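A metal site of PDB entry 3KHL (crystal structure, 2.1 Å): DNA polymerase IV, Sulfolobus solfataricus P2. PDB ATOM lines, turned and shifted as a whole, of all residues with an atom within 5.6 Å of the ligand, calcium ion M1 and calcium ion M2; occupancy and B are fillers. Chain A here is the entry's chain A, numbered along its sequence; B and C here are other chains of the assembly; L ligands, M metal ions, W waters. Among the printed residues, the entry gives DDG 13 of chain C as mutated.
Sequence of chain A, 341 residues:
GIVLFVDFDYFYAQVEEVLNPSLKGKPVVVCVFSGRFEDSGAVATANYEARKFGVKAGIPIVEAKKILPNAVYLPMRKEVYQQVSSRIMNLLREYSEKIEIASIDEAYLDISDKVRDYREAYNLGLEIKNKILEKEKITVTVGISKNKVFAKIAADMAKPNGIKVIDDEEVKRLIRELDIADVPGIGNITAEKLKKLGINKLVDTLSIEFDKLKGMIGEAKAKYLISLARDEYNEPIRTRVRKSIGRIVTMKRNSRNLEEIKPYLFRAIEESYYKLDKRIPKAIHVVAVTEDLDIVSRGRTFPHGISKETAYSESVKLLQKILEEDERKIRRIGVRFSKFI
NZ of Lys 159 is in salt-bridge range of O8 of the ligand, at 3.8 Å. A nitrogen (N2) of the ligand is in hydrogen-bond range of N1 of DA 5 of chain B (2.7 Å). The side-chain hydroxyl (OG1) of Thr 45 sits at hydrogen-bond distance from an oxygen (O5) of the ligand (2.7 Å). O7 of the ligand is in hydrogen-bond range of OH of Tyr 48, 2.8 Å away. NH1 of Arg 51 is in salt-bridge range of O8 of the ligand (2.9 Å). An oxygen (O7) of the ligand sits at hydrogen-bond distance from the backbone NH (N) of Tyr 10 (2.9 Å). The backbone NH (N) of Phe 11 lies within hydrogen-bond range of an oxygen (O5) of the ligand (3.3 Å). O12 of the ligand sits at hydrogen-bond distance from N of Tyr 12 (3.1 Å). A nitrogen (N2) of the ligand lies close to the backbone carbonyl oxygen of Ala 44 (3.4 Å).
The backbone NH of Asp 105 lies close to the side-chain hydroxyl of Ser 103 (3.2 Å). The side-chain carboxylate of Asp 7 lies within salt-bridge range of the side-chain amino group of Lys 159, 2.8 Å away. The side-chain hydroxyl (OG1) of Thr 45 sits at hydrogen-bond distance from the guanidinium group (NH2) of Arg 51 (3.1 Å). The guanidinium group (NE) of Arg 51 is in hydrogen-bond range of the backbone carbonyl oxygen (O) of Ala 46 (2.9 Å). The backbone NH (N) of Glu 106 lies close to the side-chain hydroxyl (OG) of Ser 103. OE1 of Glu 106 is in salt-bridge range of NZ of Lys 152 (3.8 Å). OP1 of DDG 13 of chain C is in salt-bridge range of the side-chain amino group of Lys 152 (3.5 Å).
An oxygen (O14) of the ligand lies close to O6 of DDG 13 of chain C, 3.3 Å away. Asp 9 touches the ligand (CA to O7, 3.9 Å). Ala 57 touches the ligand (CB to O14, 3.4 Å). Ile 104 touches the ligand. Hydrophobic or aromatic side chains that line the ligand: Phe 11, Tyr 12, Ala 44, Tyr 48, Ala 57 and Ile 104. Within 4 Å of the ligand: Asp 7, Phe 8, Asp 9, Tyr 10, Phe 11, Tyr 12, Ala 44, Thr 45, Tyr 48, Arg 51, Ala 57, Ile 104, Asp 105, Lys 159, DA 5 of chain B and DDG 13 of chain C.
Residues that only touch calcium ion M1: DDG 13 of chain C (3.3 Å). Of the 27 residues printed, 4 come within 4 Å of calcium ion M1. The nearest printed residue that does not touch calcium ion M1 is Ser 103 (4.2 Å).
Within 4 Å of calcium ion M2: Asp 7, Phe 8 and Asp 105. The nearest printed residue that does not touch calcium ion M2 is Lys 159 (4.04 Å).
Calcium ion M1 is bound by water W2 (2.1 Å), an oxygen (O1) of the ligand (2.3 Å), the side-chain carboxylate (OD1) of Asp 105 (2.5 Å), the side-chain carboxylate (OD1) of Asp 7 (2.8 Å) and the side-chain carboxylate (OE2) of Glu 106 (2.8 Å). Calcium ion M1 has five donor atoms within binding distance.
Calcium ion M2 is bound by an oxygen (O4) of the ligand, the side-chain carboxylate of Asp 105, the backbone carbonyl oxygen of Phe 8, the side-chain carboxylate of Asp 7, an oxygen (O1) of the ligand and an oxygen (O9) of the ligand.
Water W2 lies within hydrogen-bond range of OD2 of Asp 7 (2.7 Å) and NZ of Lys 159 (3.3 Å). Water W3 bridges the side-chain carboxylate (OD1) of Asp 9 (3.1 Å) and the backbone carbonyl oxygen (O) of Asp 7 (3.2 Å).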
ATOM      1  N   PHE A   5     -13.423 -29.186  13.268  1.00  0.00           N
ATOM      2  CA  PHE A   5     -13.498 -27.730  13.227  1.00  0.00           C
ATOM      3  C   PHE A   5     -13.352 -27.186  14.630  1.00  0.00           C
ATOM      4  O   PHE A   5     -13.974 -27.716  15.563  1.00  0.00           O
ATOM      5  CB  PHE A   5     -14.861 -27.335  12.651  1.00  0.00           C
ATOM      6  CG  PHE A   5     -15.161 -25.870  12.717  1.00  0.00           C
ATOM      7  CD1 PHE A   5     -14.548 -24.968  11.832  1.00  0.00           C
ATOM      8  CD2 PHE A   5     -16.095 -25.373  13.643  1.00  0.00           C
ATOM      9  CE1 PHE A   5     -14.855 -23.610  11.885  1.00  0.00           C
ATOM     10  CE2 PHE A   5     -16.388 -24.030  13.709  1.00  0.00           C
ATOM     11  CZ  PHE A   5     -15.774 -23.128  12.852  1.00  0.00           C
ATOM     12  N   ASP A   7     -13.455 -23.551  17.005  1.00  0.00           N
ATOM     13  CA  ASP A   7     -13.982 -22.187  17.059  1.00  0.00           C
ATOM     14  C   ASP A   7     -13.808 -21.776  18.526  1.00  0.00           C
ATOM     15  O   ASP A   7     -14.333 -22.457  19.410  1.00  0.00           O
ATOM     16  CB  ASP A   7     -15.477 -22.247  16.681  1.00  0.00           C
ATOM     17  CG  ASP A   7     -16.098 -20.877  16.394  1.00  0.00           C
ATOM     18  OD1 ASP A   7     -15.567 -19.847  16.853  1.00  0.00           O
ATOM     19  OD2 ASP A   7     -17.171 -20.848  15.723  1.00  0.00           O
ATOM     20  N   PHE A   8     -13.049 -20.711  18.784  1.00  0.00           N
ATOM     21  CA  PHE A   8     -12.654 -20.338  20.151  1.00  0.00           C
ATOM     22  C   PHE A   8     -13.821 -19.617  20.807  1.00  0.00           C
ATOM     23  O   PHE A   8     -14.509 -18.841  20.132  1.00  0.00           O
ATOM     24  CB  PHE A   8     -11.432 -19.395  20.158  1.00  0.00           C
ATOM     25  CG  PHE A   8     -10.265 -19.839  19.288  1.00  0.00           C
ATOM     26  CD1 PHE A   8     -10.078 -21.176  18.938  1.00  0.00           C
ATOM     27  CD2 PHE A   8      -9.309 -18.906  18.867  1.00  0.00           C
ATOM     28  CE1 PHE A   8      -9.002 -21.555  18.136  1.00  0.00           C
ATOM     29  CE2 PHE A   8      -8.210 -19.280  18.057  1.00  0.00           C
ATOM     30  CZ  PHE A   8      -8.059 -20.606  17.703  1.00  0.00           C
ATOM     31  N   ASP A   9     -14.039 -19.835  22.099  1.00  0.00           N
ATOM     32  CA  ASP A   9     -15.291 -19.318  22.727  1.00  0.00           C
ATOM     33  C   ASP A   9     -15.191 -17.845  23.042  1.00  0.00           C
ATOM     34  O   ASP A   9     -14.185 -17.400  23.579  1.00  0.00           O
ATOM     35  CB  ASP A   9     -15.701 -20.094  24.023  1.00  0.00           C
ATOM     36  CG  ASP A   9     -15.873 -21.603  23.812  1.00  0.00           C
ATOM     37  OD1 ASP A   9     -16.523 -22.081  22.868  1.00  0.00           O
ATOM     38  OD2 ASP A   9     -15.409 -22.349  24.700  1.00  0.00           O
ATOM     39  N   TYR A  10     -16.247 -17.093  22.719  1.00  0.00           N
ATOM     40  CA  TYR A  10     -16.366 -15.635  22.971  1.00  0.00           C
ATOM     41  C   TYR A  10     -15.016 -14.918  22.894  1.00  0.00           C
ATOM     42  O   TYR A  10     -14.609 -14.171  23.789  1.00  0.00           O
ATOM     43  CB  TYR A  10     -17.201 -15.332  24.267  1.00  0.00           C
ATOM     44  CG  TYR A  10     -16.675 -15.909  25.589  1.00  0.00           C
ATOM     45  CD1 TYR A  10     -16.026 -15.088  26.516  1.00  0.00           C
ATOM     46  CD2 TYR A  10     -16.808 -17.259  25.885  1.00  0.00           C
ATOM     47  CE1 TYR A  10     -15.539 -15.615  27.734  1.00  0.00           C
ATOM     48  CE2 TYR A  10     -16.312 -17.790  27.067  1.00  0.00           C
ATOM     49  CZ  TYR A  10     -15.681 -16.970  27.981  1.00  0.00           C
ATOM     50  OH  TYR A  10     -15.221 -17.526  29.123  1.00  0.00           O
ATOM     51  N   PHE A  11     -14.342 -15.139  21.765  1.00  0.00           N
ATOM     52  CA  PHE A  11     -12.877 -15.021  21.741  1.00  0.00           C
ATOM     53  C   PHE A  11     -12.247 -13.769  22.369  1.00  0.00           C
ATOM     54  O   PHE A  11     -11.458 -13.893  23.301  1.00  0.00           O
ATOM     55  CB  PHE A  11     -12.305 -15.297  20.350  1.00  0.00           C
ATOM     56  CG  PHE A  11     -10.810 -15.369  20.305  1.00  0.00           C
ATOM     57  CD1 PHE A  11     -10.111 -16.148  21.226  1.00  0.00           C
ATOM     58  CD2 PHE A  11     -10.106 -14.660  19.343  1.00  0.00           C
ATOM     59  CE1 PHE A  11      -8.714 -16.234  21.173  1.00  0.00           C
ATOM     60  CE2 PHE A  11      -8.699 -14.725  19.283  1.00  0.00           C
ATOM     61  CZ  PHE A  11      -8.008 -15.496  20.176  1.00  0.00           C
ATOM     62  N   TYR A  12     -12.590 -12.566  21.880  1.00  0.00           N
ATOM     63  CA  TYR A  12     -11.905 -11.368  22.419  1.00  0.00           C
ATOM     64  C   TYR A  12     -12.132 -11.157  23.886  1.00  0.00           C
ATOM     65  O   TYR A  12     -11.215 -10.765  24.614  1.00  0.00           O
ATOM     66  CB  TYR A  12     -12.257 -10.085  21.675  1.00  0.00           C
ATOM     67  CG  TYR A  12     -11.932 -10.055  20.199  1.00  0.00           C
ATOM     68  CD1 TYR A  12     -11.166 -11.066  19.573  1.00  0.00           C
ATOM     69  CD2 TYR A  12     -12.331  -8.958  19.410  1.00  0.00           C
ATOM     70  CE1 TYR A  12     -10.852 -10.998  18.219  1.00  0.00           C
ATOM     71  CE2 TYR A  12     -12.034  -8.879  18.064  1.00  0.00           C
ATOM     72  CZ  TYR A  12     -11.301  -9.892  17.468  1.00  0.00           C
ATOM     73  OH  TYR A  12     -11.050  -9.787  16.146  1.00  0.00           O
ATOM     74  N   ALA A  13     -13.386 -11.381  24.286  1.00  0.00           N
ATOM     75  CA  ALA A  13     -13.827 -11.295  25.670  1.00  0.00           C
ATOM     76  C   ALA A  13     -13.119 -12.319  26.550  1.00  0.00           C
ATOM     77  O   ALA A  13     -12.736 -12.021  27.691  1.00  0.00           O
ATOM     78  CB  ALA A  13     -15.359 -11.506  25.741  1.00  0.00           C
ATOM     79  N   VAL A  43     -20.120  -2.827  19.340  1.00  0.00           N
ATOM     80  CA  VAL A  43     -19.635  -4.005  20.060  1.00  0.00           C
ATOM     81  C   VAL A  43     -18.985  -5.003  19.108  1.00  0.00           C
ATOM     82  O   VAL A  43     -19.541  -5.301  18.064  1.00  0.00           O
ATOM     83  CB  VAL A  43     -20.803  -4.640  20.896  1.00  0.00           C
ATOM     84  CG1 VAL A  43     -20.447  -6.002  21.463  1.00  0.00           C
ATOM     85  CG2 VAL A  43     -21.201  -3.683  22.022  1.00  0.00           C
ATOM     86  N   ALA A  44     -17.789  -5.481  19.469  1.00  0.00           N
ATOM     87  CA  ALA A  44     -17.063  -6.519  18.747  1.00  0.00           C
ATOM     88  C   ALA A  44     -17.549  -7.898  19.202  1.00  0.00           C
ATOM     89  O   ALA A  44     -17.793  -8.789  18.389  1.00  0.00           O
ATOM     90  CB  ALA A  44     -15.530  -6.372  18.987  1.00  0.00           C
ATOM     91  N   THR A  45     -17.664  -8.062  20.515  1.00  0.00           N
ATOM     92  CA  THR A  45     -18.271  -9.275  21.091  1.00  0.00           C
ATOM     93  C   THR A  45     -18.478  -9.087  22.585  1.00  0.00           C
ATOM     94  O   THR A  45     -18.030  -8.090  23.170  1.00  0.00           O
ATOM     95  CB  THR A  45     -17.435 -10.555  20.866  1.00  0.00           C
ATOM     96  OG1 THR A  45     -18.233 -11.701  21.163  1.00  0.00           O
ATOM     97  CG2 THR A  45     -16.179 -10.579  21.757  1.00  0.00           C
ATOM     98  N   ALA A  46     -19.105 -10.064  23.217  1.00  0.00           N
ATOM     99  CA  ALA A  46     -19.323  -9.995  24.635  1.00  0.00           C
ATOM    100  C   ALA A  46     -19.315 -11.411  25.162  1.00  0.00           C
ATOM    101  O   ALA A  46     -19.547 -12.358  24.392  1.00  0.00           O
ATOM    102  CB  ALA A  46     -20.669  -9.297  24.942  1.00  0.00           C
ATOM    103  N   TYR A  48     -20.707 -14.606  27.543  1.00  0.00           N
ATOM    104  CA  TYR A  48     -22.044 -15.159  27.590  1.00  0.00           C
ATOM    105  C   TYR A  48     -22.900 -14.494  28.665  1.00  0.00           C
ATOM    106  O   TYR A  48     -24.104 -14.334  28.463  1.00  0.00           O
ATOM    107  CB  TYR A  48     -22.006 -16.685  27.713  1.00  0.00           C
ATOM    108  CG  TYR A  48     -21.777 -17.346  26.362  1.00  0.00           C
ATOM    109  CD1 TYR A  48     -20.502 -17.362  25.771  1.00  0.00           C
ATOM    110  CD2 TYR A  48     -22.848 -17.909  25.632  1.00  0.00           C
ATOM    111  CE1 TYR A  48     -20.271 -17.936  24.512  1.00  0.00           C
ATOM    112  CE2 TYR A  48     -22.618 -18.495  24.352  1.00  0.00           C
ATOM    113  CZ  TYR A  48     -21.322 -18.498  23.823  1.00  0.00           C
ATOM    114  OH  TYR A  48     -21.065 -19.067  22.612  1.00  0.00           O
ATOM    115  N   ARG A  51     -24.335 -11.551  27.033  1.00  0.00           N
ATOM    116  CA  ARG A  51     -25.298 -11.939  25.996  1.00  0.00           C
ATOM    117  C   ARG A  51     -26.695 -12.268  26.506  1.00  0.00           C
ATOM    118  O   ARG A  51     -27.672 -12.034  25.778  1.00  0.00           O
ATOM    119  CB  ARG A  51     -24.810 -13.108  25.171  1.00  0.00           C
ATOM    120  CG  ARG A  51     -23.545 -12.794  24.415  1.00  0.00           C
ATOM    121  CD  ARG A  51     -23.170 -13.920  23.512  1.00  0.00           C
ATOM    122  NE  ARG A  51     -21.767 -13.757  23.137  1.00  0.00           N
ATOM    123  CZ  ARG A  51     -21.099 -14.517  22.282  1.00  0.00           C
ATOM    124  NH1 ARG A  51     -21.704 -15.547  21.680  1.00  0.00           N
ATOM    125  NH2 ARG A  51     -19.818 -14.253  22.057  1.00  0.00           N
ATOM    126  N   ALA A  57     -22.266  -8.885  19.236  1.00  0.00           N
ATOM    127  CA  ALA A  57     -21.496  -8.308  18.137  1.00  0.00           C
ATOM    128  C   ALA A  57     -22.383  -7.485  17.221  1.00  0.00           C
ATOM    129  O   ALA A  57     -23.452  -7.924  16.858  1.00  0.00           O
ATOM    130  CB  ALA A  57     -20.788  -9.408  17.366  1.00  0.00           C
ATOM    131  N   GLY A  58     -21.956  -6.272  16.884  1.00  0.00           N
ATOM    132  CA  GLY A  58     -22.672  -5.441  15.928  1.00  0.00           C
ATOM    133  C   GLY A  58     -23.456  -4.276  16.483  1.00  0.00           C
ATOM    134  O   GLY A  58     -23.598  -3.252  15.826  1.00  0.00           O
ATOM    135  N   MET A  76     -11.311  -2.674  22.227  1.00  0.00           N
ATOM    136  CA  MET A  76     -10.800  -3.829  21.506  1.00  0.00           C
ATOM    137  C   MET A  76      -9.284  -3.688  21.329  1.00  0.00           C
ATOM    138  O   MET A  76      -8.805  -2.645  20.877  1.00  0.00           O
ATOM    139  CB  MET A  76     -11.491  -3.963  20.130  1.00  0.00           C
ATOM    140  CG  MET A  76     -11.057  -5.187  19.329  1.00  0.00           C
ATOM    141  SD  MET A  76     -11.535  -5.088  17.604  1.00  0.00           S
ATOM    142  CE  MET A  76     -10.734  -3.595  17.013  1.00  0.00           C
ATOM    143  N   SER A 103     -10.596 -17.830  10.074  1.00  0.00           N
ATOM    144  CA  SER A 103     -10.798 -16.517  10.694  1.00  0.00           C
ATOM    145  C   SER A 103      -9.827 -16.345  11.866  1.00  0.00           C
ATOM    146  O   SER A 103      -9.010 -17.243  12.143  1.00  0.00           O
ATOM    147  CB  SER A 103     -12.247 -16.338  11.154  1.00  0.00           C
ATOM    148  OG  SER A 103     -12.523 -17.054  12.348  1.00  0.00           O
ATOM    149  N   ILE A 104      -9.926 -15.223  12.580  1.00  0.00           N
ATOM    150  CA  ILE A 104      -9.091 -15.017  13.748  1.00  0.00           C
ATOM    151  C   ILE A 104      -9.276 -16.125  14.804  1.00  0.00           C
ATOM    152  O   ILE A 104      -8.419 -16.320  15.661  1.00  0.00           O
ATOM    153  CB  ILE A 104      -9.253 -13.596  14.350  1.00  0.00           C
ATOM    154  CG1 ILE A 104      -8.076 -13.251  15.280  1.00  0.00           C
ATOM    155  CG2 ILE A 104     -10.614 -13.424  15.067  1.00  0.00           C
ATOM    156  CD1 ILE A 104      -7.849 -11.727  15.537  1.00  0.00           C
ATOM    157  N   ASP A 105     -10.380 -16.872  14.722  1.00  0.00           N
ATOM    158  CA  ASP A 105     -10.681 -17.843  15.792  1.00  0.00           C
ATOM    159  C   ASP A 105     -11.282 -19.170  15.369  1.00  0.00           C
ATOM    160  O   ASP A 105     -11.936 -19.845  16.156  1.00  0.00           O
ATOM    161  CB  ASP A 105     -11.531 -17.173  16.888  1.00  0.00           C
ATOM    162  CG  ASP A 105     -13.028 -17.306  16.666  1.00  0.00           C
ATOM    163  OD1 ASP A 105     -13.504 -17.281  15.500  1.00  0.00           O
ATOM    164  OD2 ASP A 105     -13.739 -17.476  17.666  1.00  0.00           O
ATOM    165  N   GLU A 106     -11.079 -19.537  14.103  1.00  0.00           N
ATOM    166  CA  GLU A 106     -11.683 -20.719  13.481  1.00  0.00           C
ATOM    167  C   GLU A 106     -10.646 -21.419  12.642  1.00  0.00           C
ATOM    168  O   GLU A 106      -9.907 -20.755  11.906  1.00  0.00           O
ATOM    169  CB  GLU A 106     -12.776 -20.283  12.496  1.00  0.00           C
ATOM    170  CG  GLU A 106     -14.122 -20.081  13.105  1.00  0.00           C
ATOM    171  CD  GLU A 106     -15.205 -19.788  12.071  1.00  0.00           C
ATOM    172  OE1 GLU A 106     -14.943 -19.882  10.856  1.00  0.00           O
ATOM    173  OE2 GLU A 106     -16.337 -19.512  12.495  1.00  0.00           O
ATOM    174  N   LYS A 152     -18.872 -27.431  11.135  1.00  0.00           N
ATOM    175  CA  LYS A 152     -19.122 -26.100  11.652  1.00  0.00           C
ATOM    176  C   LYS A 152     -20.481 -26.026  12.340  1.00  0.00           C
ATOM    177  O   LYS A 152     -20.622 -25.424  13.409  1.00  0.00           O
ATOM    178  CB  LYS A 152     -19.019 -25.029  10.559  1.00  0.00           C
ATOM    179  CG  LYS A 152     -19.336 -23.624  11.088  1.00  0.00           C
ATOM    180  CD  LYS A 152     -19.337 -22.607   9.960  1.00  0.00           C
ATOM    181  CE  LYS A 152     -18.251 -21.575  10.154  1.00  0.00           C
ATOM    182  NZ  LYS A 152     -18.626 -20.636  11.271  1.00  0.00           N
ATOM    183  N   LYS A 159     -21.571 -25.029  21.240  1.00  0.00           N
ATOM    184  CA  LYS A 159     -21.055 -23.762  21.825  1.00  0.00           C
ATOM    185  C   LYS A 159     -21.758 -23.383  23.147  1.00  0.00           C
ATOM    186  O   LYS A 159     -22.953 -23.430  23.180  1.00  0.00           O
ATOM    187  CB  LYS A 159     -21.343 -22.596  20.844  1.00  0.00           C
ATOM    188  CG  LYS A 159     -20.250 -22.304  19.838  1.00  0.00           C
ATOM    189  CD  LYS A 159     -20.503 -21.041  19.016  1.00  0.00           C
ATOM    190  CE  LYS A 159     -19.592 -21.046  17.784  1.00  0.00           C
ATOM    191  NZ  LYS A 159     -19.322 -19.698  17.124  1.00  0.00           N
ATOM    192  N   PRO A 160     -21.025 -22.921  24.191  1.00  0.00           N
ATOM    193  CA  PRO A 160     -19.555 -22.757  24.372  1.00  0.00           C
ATOM    194  C   PRO A 160     -18.903 -23.956  25.060  1.00  0.00           C
ATOM    195  O   PRO A 160     -19.593 -24.789  25.638  1.00  0.00           O
ATOM    196  CB  PRO A 160     -19.453 -21.526  25.299  1.00  0.00           C
ATOM    197  CG  PRO A 160     -20.679 -21.677  26.228  1.00  0.00           C
ATOM    198  CD  PRO A 160     -21.780 -22.227  25.258  1.00  0.00           C
ATOM    199  P    DA B   5     -20.246   2.089  12.585  1.00  0.00           P
ATOM    200  OP1  DA B   5     -20.000   3.552  12.578  1.00  0.00           O
ATOM    201  OP2  DA B   5     -20.460   1.370  11.315  1.00  0.00           O
ATOM    202  O5'  DA B   5     -19.013   1.405  13.334  1.00  0.00           O
ATOM    203  C5'  DA B   5     -18.429   2.012  14.494  1.00  0.00           C
ATOM    204  C4'  DA B   5     -17.060   1.398  14.667  1.00  0.00           C
ATOM    205  O4'  DA B   5     -17.169   0.000  15.018  1.00  0.00           O
ATOM    206  C3'  DA B   5     -16.191   1.424  13.423  1.00  0.00           C
ATOM    207  O3'  DA B   5     -14.871   1.561  13.849  1.00  0.00           O
ATOM    208  C2'  DA B   5     -16.399   0.045  12.782  1.00  0.00           C
ATOM    209  C1'  DA B   5     -16.642  -0.824  14.003  1.00  0.00           C
ATOM    210  N9   DA B   5     -17.633  -1.896  13.824  1.00  0.00           N
ATOM    211  C8   DA B   5     -18.906  -1.814  13.330  1.00  0.00           C
ATOM    212  N7   DA B   5     -19.533  -2.966  13.325  1.00  0.00           N
ATOM    213  C5   DA B   5     -18.618  -3.862  13.843  1.00  0.00           C
ATOM    214  C6   DA B   5     -18.652  -5.261  14.112  1.00  0.00           C
ATOM    215  N6   DA B   5     -19.693  -6.078  13.885  1.00  0.00           N
ATOM    216  N1   DA B   5     -17.522  -5.811  14.640  1.00  0.00           N
ATOM    217  C2   DA B   5     -16.458  -5.054  14.902  1.00  0.00           C
ATOM    218  N3   DA B   5     -16.311  -3.735  14.704  1.00  0.00           N
ATOM    219  C4   DA B   5     -17.440  -3.209  14.161  1.00  0.00           C
ATOM    220  P    DC B   6     -13.725   2.108  12.880  1.00  0.00           P
ATOM    221  OP1  DC B   6     -12.760   2.757  13.801  1.00  0.00           O
ATOM    222  OP2  DC B   6     -14.343   2.882  11.782  1.00  0.00           O
ATOM    223  O5'  DC B   6     -13.115   0.759  12.274  1.00  0.00           O
ATOM    224  C5'  DC B   6     -12.509  -0.131  13.189  1.00  0.00           C
ATOM    225  C4'  DC B   6     -12.552  -1.537  12.657  1.00  0.00           C
ATOM    226  O4'  DC B   6     -13.910  -1.986  12.548  1.00  0.00           O
ATOM    227  C3'  DC B   6     -11.970  -1.666  11.250  1.00  0.00           C
ATOM    228  O3'  DC B   6     -10.712  -2.277  11.416  1.00  0.00           O
ATOM    229  C2'  DC B   6     -12.975  -2.544  10.503  1.00  0.00           C
ATOM    230  C1'  DC B   6     -13.820  -3.056  11.657  1.00  0.00           C
ATOM    231  N1   DC B   6     -15.157  -3.565  11.313  1.00  0.00           N
ATOM    232  C2   DC B   6     -15.414  -4.913  11.660  1.00  0.00           C
ATOM    233  O2   DC B   6     -14.531  -5.582  12.221  1.00  0.00           O
ATOM    234  N3   DC B   6     -16.614  -5.445  11.357  1.00  0.00           N
ATOM    235  C4   DC B   6     -17.539  -4.704  10.742  1.00  0.00           C
ATOM    236  N4   DC B   6     -18.687  -5.310  10.471  1.00  0.00           N
ATOM    237  C5   DC B   6     -17.308  -3.325  10.382  1.00  0.00           C
ATOM    238  C6   DC B   6     -16.103  -2.802  10.671  1.00  0.00           C
ATOM    239  P   DDG C  13     -19.346 -16.845  11.618  1.00  0.00           P
ATOM    240  OP1 DDG C  13     -18.930 -17.555  12.842  1.00  0.00           O
ATOM    241  OP2 DDG C  13     -20.496 -15.905  11.662  1.00  0.00           O
ATOM    242  O5' DDG C  13     -18.103 -16.034  10.988  1.00  0.00           O
ATOM    243  C5' DDG C  13     -16.804 -16.627  10.910  1.00  0.00           C
ATOM    244  C4' DDG C  13     -15.745 -15.628  11.347  1.00  0.00           C
ATOM    245  O4' DDG C  13     -15.900 -14.405  10.568  1.00  0.00           O
ATOM    246  C3' DDG C  13     -15.780 -15.215  12.820  1.00  0.00           C
ATOM    247  C2' DDG C  13     -15.372 -13.740  12.823  1.00  0.00           C
ATOM    248  C1' DDG C  13     -15.668 -13.282  11.387  1.00  0.00           C
ATOM    249  N9  DDG C  13     -16.786 -12.333  11.230  1.00  0.00           N
ATOM    250  C8  DDG C  13     -18.104 -12.535  10.876  1.00  0.00           C
ATOM    251  N7  DDG C  13     -18.788 -11.417  10.829  1.00  0.00           N
ATOM    252  C5  DDG C  13     -17.872 -10.421  11.142  1.00  0.00           C
ATOM    253  C6  DDG C  13     -17.992  -9.009  11.245  1.00  0.00           C
ATOM    254  O6  DDG C  13     -18.997  -8.287  11.061  1.00  0.00           O
ATOM    255  N1  DDG C  13     -16.781  -8.407  11.597  1.00  0.00           N
ATOM    256  C2  DDG C  13     -15.596  -9.079  11.825  1.00  0.00           C
ATOM    257  N2  DDG C  13     -14.519  -8.366  12.164  1.00  0.00           N
ATOM    258  N3  DDG C  13     -15.486 -10.386  11.735  1.00  0.00           N
ATOM    259  C4  DDG C  13     -16.639 -10.980  11.387  1.00  0.00           C
HETATM  260  P1  LIG L   1     -17.212 -15.406  16.599  1.00  0.00           P
HETATM  261  O1  LIG L   1     -16.664 -16.809  16.657  1.00  0.00           O
HETATM  262  O2  LIG L   1     -18.392 -15.207  15.686  1.00  0.00           O
HETATM  263  O3  LIG L   1     -17.765 -14.875  18.029  1.00  0.00           O
HETATM  264  P2  LIG L   1     -17.177 -15.220  19.501  1.00  0.00           P
HETATM  265  O4  LIG L   1     -15.977 -16.137  19.518  1.00  0.00           O
HETATM  266  O5  LIG L   1     -16.924 -13.884  20.175  1.00  0.00           O
HETATM  267  O6  LIG L   1     -18.407 -15.887  20.264  1.00  0.00           O
HETATM  268  P3  LIG L   1     -18.918 -17.413  20.148  1.00  0.00           P
HETATM  269  O7  LIG L   1     -18.723 -18.097  21.480  1.00  0.00           O
HETATM  270  O8  LIG L   1     -20.405 -17.423  19.925  1.00  0.00           O
HETATM  271  O9  LIG L   1     -18.182 -18.251  19.133  1.00  0.00           O
HETATM  272  O10 LIG L   1     -16.056 -14.344  16.228  1.00  0.00           O
HETATM  273  C1  LIG L   1     -14.761 -14.400  16.820  1.00  0.00           C
HETATM  274  C2  LIG L   1     -14.223 -13.002  17.133  1.00  0.00           C
HETATM  275  O11 LIG L   1     -14.234 -12.133  16.008  1.00  0.00           O
HETATM  276  C3  LIG L   1     -15.037 -12.290  18.198  1.00  0.00           C
HETATM  277  O12 LIG L   1     -14.614 -12.668  19.511  1.00  0.00           O
HETATM  278  C4  LIG L   1     -14.771 -10.823  17.899  1.00  0.00           C
HETATM  279  C5  LIG L   1     -14.595 -10.792  16.362  1.00  0.00           C
HETATM  280  N1  LIG L   1     -15.890 -10.344  15.796  1.00  0.00           N
HETATM  281  C6  LIG L   1     -16.089  -8.965  15.587  1.00  0.00           C
HETATM  282  O13 LIG L   1     -15.167  -8.141  15.857  1.00  0.00           O
HETATM  283  N2  LIG L   1     -17.242  -8.485  15.095  1.00  0.00           N
HETATM  284  C7  LIG L   1     -18.271  -9.302  14.797  1.00  0.00           C
HETATM  285  O14 LIG L   1     -19.341  -8.834  14.328  1.00  0.00           O
HETATM  286  C8  LIG L   1     -18.107 -10.772  15.023  1.00  0.00           C
HETATM  287  C9  LIG L   1     -19.225 -11.721  14.682  1.00  0.00           C
HETATM  288  C10 LIG L   1     -16.885 -11.224  15.524  1.00  0.00           C
HETATM  289 CA    CA M   1     -15.805 -17.918  14.792  1.00  0.00          CA
HETATM  290 CA    CA M   2     -15.824 -18.125  18.381  1.00  0.00          CA
HETATM  291  O   HOH W   1     -21.658  -9.554  13.479  1.00  0.00           O
HETATM  292  O   HOH W   2     -17.741 -18.576  14.399  1.00  0.00           O
HETATM  293  O   HOH W   3     -17.228 -21.168  20.039  1.00  0.00           O
